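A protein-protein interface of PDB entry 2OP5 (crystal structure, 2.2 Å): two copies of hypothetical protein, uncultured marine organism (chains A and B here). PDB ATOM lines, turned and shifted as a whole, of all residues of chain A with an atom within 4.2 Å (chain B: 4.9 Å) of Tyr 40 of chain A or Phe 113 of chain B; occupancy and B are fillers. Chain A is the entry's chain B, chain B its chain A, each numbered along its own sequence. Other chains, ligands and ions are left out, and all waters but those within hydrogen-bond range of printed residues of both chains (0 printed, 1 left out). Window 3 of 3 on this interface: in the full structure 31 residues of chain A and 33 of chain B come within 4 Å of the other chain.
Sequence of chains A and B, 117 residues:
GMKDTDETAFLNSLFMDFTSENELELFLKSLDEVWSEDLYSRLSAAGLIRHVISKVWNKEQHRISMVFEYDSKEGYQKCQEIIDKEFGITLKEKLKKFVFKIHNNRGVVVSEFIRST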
ATOM      1  N   TRP A  35      12.576  -8.567   6.219  1.00  0.00           N
ATOM      2  CA  TRP A  35      12.591  -7.540   5.184  1.00  0.00           C
ATOM      3  C   TRP A  35      13.786  -7.832   4.323  1.00  0.00           C
ATOM      4  O   TRP A  35      14.812  -7.153   4.401  1.00  0.00           O
ATOM      5  CB  TRP A  35      12.692  -6.162   5.814  1.00  0.00           C
ATOM      6  CG  TRP A  35      11.466  -5.855   6.525  1.00  0.00           C
ATOM      7  CD1 TRP A  35      11.194  -6.087   7.832  1.00  0.00           C
ATOM      8  CD2 TRP A  35      10.291  -5.312   5.950  1.00  0.00           C
ATOM      9  NE1 TRP A  35       9.914  -5.694   8.116  1.00  0.00           N
ATOM     10  CE2 TRP A  35       9.337  -5.213   6.973  1.00  0.00           C
ATOM     11  CE3 TRP A  35       9.953  -4.884   4.657  1.00  0.00           C
ATOM     12  CZ2 TRP A  35       8.062  -4.724   6.752  1.00  0.00           C
ATOM     13  CZ3 TRP A  35       8.699  -4.377   4.446  1.00  0.00           C
ATOM     14  CH2 TRP A  35       7.763  -4.300   5.491  1.00  0.00           C
ATOM     15  N   SER A  36      13.631  -8.870   3.508  1.00  0.00           N
ATOM     16  CA  SER A  36      14.693  -9.367   2.670  1.00  0.00           C
ATOM     17  C   SER A  36      14.887  -8.498   1.441  1.00  0.00           C
ATOM     18  O   SER A  36      14.056  -7.635   1.147  1.00  0.00           O
ATOM     19  CB  SER A  36      14.408 -10.825   2.271  1.00  0.00           C
ATOM     20  OG  SER A  36      13.260 -10.941   1.446  1.00  0.00           O
ATOM     21  N   GLU A  37      16.002  -8.735   0.744  1.00  0.00           N
ATOM     22  CA  GLU A  37      16.350  -7.998  -0.467  1.00  0.00           C
ATOM     23  C   GLU A  37      15.323  -8.254  -1.556  1.00  0.00           C
ATOM     24  O   GLU A  37      14.964  -7.358  -2.328  1.00  0.00           O
ATOM     25  CB  GLU A  37      17.727  -8.435  -0.972  1.00  0.00           C
ATOM     26  N   ASP A  38      14.859  -9.496  -1.609  1.00  0.00           N
ATOM     27  CA  ASP A  38      13.877  -9.910  -2.591  1.00  0.00           C
ATOM     28  C   ASP A  38      12.574  -9.120  -2.417  1.00  0.00           C
ATOM     29  O   ASP A  38      11.998  -8.608  -3.393  1.00  0.00           O
ATOM     30  CB  ASP A  38      13.627 -11.407  -2.451  1.00  0.00           C
ATOM     31  CG  ASP A  38      13.054 -12.010  -3.694  1.00  0.00           C
ATOM     32  OD1 ASP A  38      12.038 -11.486  -4.205  1.00  0.00           O
ATOM     33  OD2 ASP A  38      13.627 -13.023  -4.155  1.00  0.00           O
ATOM     34  N   LEU A  39      12.123  -9.022  -1.171  1.00  0.00           N
ATOM     35  CA  LEU A  39      10.914  -8.272  -0.860  1.00  0.00           C
ATOM     36  C   LEU A  39      11.072  -6.807  -1.257  1.00  0.00           C
ATOM     37  O   LEU A  39      10.179  -6.239  -1.862  1.00  0.00           O
ATOM     38  CB  LEU A  39      10.557  -8.390   0.621  1.00  0.00           C
ATOM     39  CG  LEU A  39       9.248  -7.698   1.006  1.00  0.00           C
ATOM     40  CD1 LEU A  39       8.075  -8.335   0.314  1.00  0.00           C
ATOM     41  CD2 LEU A  39       9.053  -7.673   2.542  1.00  0.00           C
ATOM     42  N   TYR A  40      12.203  -6.202  -0.915  1.00  0.00           N
ATOM     43  CA  TYR A  40      12.445  -4.799  -1.280  1.00  0.00           C
ATOM     44  C   TYR A  40      12.534  -4.588  -2.789  1.00  0.00           C
ATOM     45  O   TYR A  40      12.171  -3.521  -3.276  1.00  0.00           O
ATOM     46  CB  TYR A  40      13.723  -4.258  -0.644  1.00  0.00           C
ATOM     47  CG  TYR A  40      13.594  -3.865   0.804  1.00  0.00           C
ATOM     48  CD1 TYR A  40      12.742  -2.825   1.176  1.00  0.00           C
ATOM     49  CD2 TYR A  40      14.354  -4.468   1.791  1.00  0.00           C
ATOM     50  CE1 TYR A  40      12.623  -2.430   2.476  1.00  0.00           C
ATOM     51  CE2 TYR A  40      14.234  -4.055   3.125  1.00  0.00           C
ATOM     52  CZ  TYR A  40      13.381  -3.039   3.447  1.00  0.00           C
ATOM     53  OH  TYR A  40      13.232  -2.608   4.739  1.00  0.00           O
ATOM     54  N   SER A  41      13.043  -5.575  -3.520  1.00  0.00           N
ATOM     55  CA  SER A  41      13.113  -5.474  -4.982  1.00  0.00           C
ATOM     56  C   SER A  41      11.698  -5.361  -5.522  1.00  0.00           C
ATOM     57  O   SER A  41      11.425  -4.531  -6.374  1.00  0.00           O
ATOM     58  CB  SER A  41      13.813  -6.690  -5.602  1.00  0.00           C
ATOM     59  N   ARG A  42      10.804  -6.191  -4.995  1.00  0.00           N
ATOM     60  CA  ARG A  42       9.399  -6.202  -5.406  1.00  0.00           C
ATOM     61  C   ARG A  42       8.614  -4.947  -4.994  1.00  0.00           C
ATOM     62  O   ARG A  42       7.837  -4.403  -5.777  1.00  0.00           O
ATOM     63  CB  ARG A  42       8.706  -7.468  -4.872  1.00  0.00           C
ATOM     64  CG  ARG A  42       9.124  -8.717  -5.625  1.00  0.00           C
ATOM     65  CD  ARG A  42       8.320  -9.956  -5.250  1.00  0.00           C
ATOM     66  NE  ARG A  42       8.814 -10.631  -4.048  1.00  0.00           N
ATOM     67  CZ  ARG A  42       8.239 -10.639  -2.843  1.00  0.00           C
ATOM     68  NH1 ARG A  42       7.088 -10.007  -2.610  1.00  0.00           N
ATOM     69  NH2 ARG A  42       8.823 -11.325  -1.854  1.00  0.00           N
ATOM     70  N   LEU A  43       8.813  -4.503  -3.763  1.00  0.00           N
ATOM     71  CA  LEU A  43       8.143  -3.312  -3.262  1.00  0.00           C
ATOM     72  C   LEU A  43       8.670  -2.056  -3.941  1.00  0.00           C
ATOM     73  O   LEU A  43       7.912  -1.128  -4.203  1.00  0.00           O
ATOM     74  CB  LEU A  43       8.317  -3.215  -1.747  1.00  0.00           C
ATOM     75  CG  LEU A  43       7.665  -4.331  -0.937  1.00  0.00           C
ATOM     76  CD1 LEU A  43       8.078  -4.257   0.501  1.00  0.00           C
ATOM     77  CD2 LEU A  43       6.171  -4.235  -1.048  1.00  0.00           C
ATOM     78  N   SER A  44       9.973  -2.029  -4.192  1.00  0.00           N
ATOM     79  CA  SER A  44      10.623  -0.916  -4.867  1.00  0.00           C
ATOM     80  C   SER A  44       9.976  -0.692  -6.228  1.00  0.00           C
ATOM     81  O   SER A  44       9.470   0.405  -6.524  1.00  0.00           O
ATOM     82  CB  SER A  44      12.117  -1.217  -5.037  1.00  0.00           C
ATOM     83  OG  SER A  44      12.792  -0.211  -5.758  1.00  0.00           O
ATOM     84  N   LEU A  48       7.383   1.703  -3.677  1.00  0.00           N
ATOM     85  CA  LEU A  48       8.019   2.040  -2.399  1.00  0.00           C
ATOM     86  C   LEU A  48       9.242   2.924  -2.609  1.00  0.00           C
ATOM     87  O   LEU A  48      10.173   2.548  -3.314  1.00  0.00           O
ATOM     88  CB  LEU A  48       8.425   0.769  -1.652  1.00  0.00           C
ATOM     89  CG  LEU A  48       9.096   0.905  -0.281  1.00  0.00           C
ATOM     90  CD1 LEU A  48       8.159   1.540   0.731  1.00  0.00           C
ATOM     91  CD2 LEU A  48       9.569  -0.445   0.222  1.00  0.00           C
ATOM     92  N   ARG A  50      10.880   4.765   0.260  1.00  0.00           N
ATOM     93  CA  ARG A  50      11.719   4.666   1.446  1.00  0.00           C
ATOM     94  C   ARG A  50      11.074   3.811   2.500  1.00  0.00           C
ATOM     95  O   ARG A  50       9.853   3.660   2.546  1.00  0.00           O
ATOM     96  CB  ARG A  50      11.910   6.043   2.115  1.00  0.00           C
ATOM     97  CG  ARG A  50      12.572   7.071   1.260  1.00  0.00           C
ATOM     98  CD  ARG A  50      12.586   8.477   1.877  1.00  0.00           C
ATOM     99  NE  ARG A  50      13.749   8.669   2.740  1.00  0.00           N
ATOM    100  CZ  ARG A  50      13.764   8.613   4.076  1.00  0.00           C
ATOM    101  NH1 ARG A  50      12.656   8.406   4.796  1.00  0.00           N
ATOM    102  NH2 ARG A  50      14.920   8.811   4.696  1.00  0.00           N
ATOM    103  N   HIS A  51      11.933   3.278   3.356  1.00  0.00           N
ATOM    104  CA  HIS A  51      11.518   2.524   4.526  1.00  0.00           C
ATOM    105  C   HIS A  51      12.585   2.707   5.604  1.00  0.00           C
ATOM    106  O   HIS A  51      13.751   2.372   5.395  1.00  0.00           O
ATOM    107  CB  HIS A  51      11.289   1.051   4.219  1.00  0.00           C
ATOM    108  CG  HIS A  51      10.794   0.269   5.400  1.00  0.00           C
ATOM    109  ND1 HIS A  51      11.276  -0.982   5.724  1.00  0.00           N
ATOM    110  CD2 HIS A  51       9.891   0.588   6.359  1.00  0.00           C
ATOM    111  CE1 HIS A  51      10.665  -1.415   6.811  1.00  0.00           C
ATOM    112  NE2 HIS A  51       9.826  -0.479   7.222  1.00  0.00           N
ATOM    113  N   SER B 111      17.639   0.651  10.517  1.00  0.00           N
ATOM    114  CA  SER B 111      17.712   0.248   9.128  1.00  0.00           C
ATOM    115  C   SER B 111      17.002   1.286   8.286  1.00  0.00           C
ATOM    116  O   SER B 111      15.974   1.858   8.704  1.00  0.00           O
ATOM    117  CB  SER B 111      17.067  -1.124   8.944  1.00  0.00           C
ATOM    118  OG  SER B 111      17.301  -1.632   7.653  1.00  0.00           O
ATOM    119  N   GLU B 112      17.573   1.543   7.115  1.00  0.00           N
ATOM    120  CA  GLU B 112      17.025   2.487   6.154  1.00  0.00           C
ATOM    121  C   GLU B 112      17.192   1.981   4.707  1.00  0.00           C
ATOM    122  O   GLU B 112      18.307   1.700   4.248  1.00  0.00           O
ATOM    123  CB  GLU B 112      17.700   3.851   6.278  1.00  0.00           C
ATOM    124  CG  GLU B 112      16.971   4.954   5.498  1.00  0.00           C
ATOM    125  CD  GLU B 112      17.640   6.311   5.598  1.00  0.00           C
ATOM    126  OE1 GLU B 112      18.686   6.434   6.289  1.00  0.00           O
ATOM    127  OE2 GLU B 112      17.116   7.252   4.968  1.00  0.00           O
ATOM    128  N   PHE B 113      16.061   1.846   4.021  1.00  0.00           N
ATOM    129  CA  PHE B 113      16.048   1.530   2.621  1.00  0.00           C
ATOM    130  C   PHE B 113      15.558   2.740   1.855  1.00  0.00           C
ATOM    131  O   PHE B 113      14.545   3.326   2.206  1.00  0.00           O
ATOM    132  CB  PHE B 113      15.144   0.368   2.300  1.00  0.00           C
ATOM    133  CG  PHE B 113      15.003   0.145   0.832  1.00  0.00           C
ATOM    134  CD1 PHE B 113      16.048  -0.384   0.102  1.00  0.00           C
ATOM    135  CD2 PHE B 113      13.833   0.491   0.164  1.00  0.00           C
ATOM    136  CE1 PHE B 113      15.913  -0.595  -1.274  1.00  0.00           C
ATOM    137  CE2 PHE B 113      13.701   0.291  -1.205  1.00  0.00           C
ATOM    138  CZ  PHE B 113      14.737  -0.246  -1.918  1.00  0.00           C
ATOM    139  N   ILE B 114      16.292   3.095   0.809  1.00  0.00           N
ATOM    140  CA  ILE B 114      15.979   4.206  -0.071  1.00  0.00           C
ATOM    141  C   ILE B 114      15.998   3.599  -1.470  1.00  0.00           C
ATOM    142  O   ILE B 114      16.879   2.792  -1.761  1.00  0.00           O
ATOM    143  CB  ILE B 114      17.043   5.304   0.042  1.00  0.00           C
ATOM    144  CG1 ILE B 114      17.437   5.519   1.510  1.00  0.00           C
ATOM    145  CG2 ILE B 114      16.522   6.603  -0.593  1.00  0.00           C
ATOM    146  CD1 ILE B 114      18.594   6.509   1.713  1.00  0.00           C
ATOM    147  N   ARG B 115      15.039   3.957  -2.326  1.00  0.00           N
ATOM    148  CA  ARG B 115      14.923   3.335  -3.675  1.00  0.00           C
ATOM    149  C   ARG B 115      16.042   3.747  -4.649  1.00  0.00           C
ATOM    150  O   ARG B 115      16.451   4.919  -4.668  1.00  0.00           O
ATOM    151  CB  ARG B 115      13.538   3.619  -4.281  1.00  0.00           C
ATOM    152  CG  ARG B 115      13.361   3.118  -5.697  1.00  0.00           C
ATOM    153  CD  ARG B 115      11.892   3.001  -6.119  1.00  0.00           C
ATOM    154  NE  ARG B 115      11.243   4.290  -6.342  1.00  0.00           N
ATOM    155  CZ  ARG B 115       9.973   4.438  -6.725  1.00  0.00           C
ATOM    156  NH1 ARG B 115       9.182   3.389  -6.908  1.00  0.00           N
ATOM    157  NH2 ARG B 115       9.478   5.649  -6.919  1.00  0.00           N
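The guanidinium group (NH2) of Arg 50 of chain A is in salt-bridge range of the side-chain carboxylate (OE2) of Glu 112 of chain B (2.7 Å).
N of Phe 113 of chain B sits at hydrogen-bond distance from O of His 51 of chain A.
The guanidinium group (NH1) of Arg 115 of chain B is in hydrogen-bond range of the backbone carbonyl oxygen (O) of Ser 44 of chain A.
No position is printed for both chains.
Printed residues of chain A that touch a printed residue of chain B: Tyr 40, Ser 44, Leu 48, Arg 50 and His 51.
Hydrophobic or aromatic side chains of chain A within 4 Å of the printed part of chain B: Tyr 40.
Of the 5 printed residues of chain B, 3 touch a printed residue of chain A.
Hydrophobic or aromatic side chains of chain B that line the printed part of chain A: Phe 113.
Among the printed residues, Asp or Glu carboxylates within 4 Å of a Lys or Arg side-chain nitrogen of the other chain: Arg 50 of chain A with Glu 112 of chain B (2.7 Å).
Among the printed residues, merely in contact across the chains: Arg 50 of chain A with Phe 113 of chain B, Leu 48 of chain A with Arg 115 of chain B, His 51 of chain A with Glu 112 of chain B and Tyr 40 of chain A with Phe 113 of chain B.
Of chain B, only Phe 113 comes within 4 Å of Tyr 40 of chain A.
Printed residues of chain B within 4 Å of Arg 50 of chain A: Glu 112 (2.7 Å) and Phe 113 (3.2 Å).
Of the printed residues of chain A, Glu 112 of chain B touches Arg 50 (2.7 Å) and His 51 (3.4 Å).
Phe 113 of chain B touches three residues of chain A.
Printed residues of chain A within 4 Å of Arg 115 of chain B: Ser 44 and Leu 48.
The nearest printed residue of chain B that does not touch Tyr 40 of chain A is Ser 111 of chain B (5.1 Å).
The nearest printed residue of chain B that does not touch Ser 44 of chain A is Phe 113 of chain B (4.2 Å).
The backbone carbonyl oxygen (O) of Leu 43 of chain A is in hydrogen-bond range of the backbone NH (N) of Leu 48 of chain A, 2.9 Å away.
The side-chain hydroxyl (OH) of Tyr 40 of chain A lies within hydrogen-bond range of a ring nitrogen (ND1) of His 51 of chain A, 2.7 Å away.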
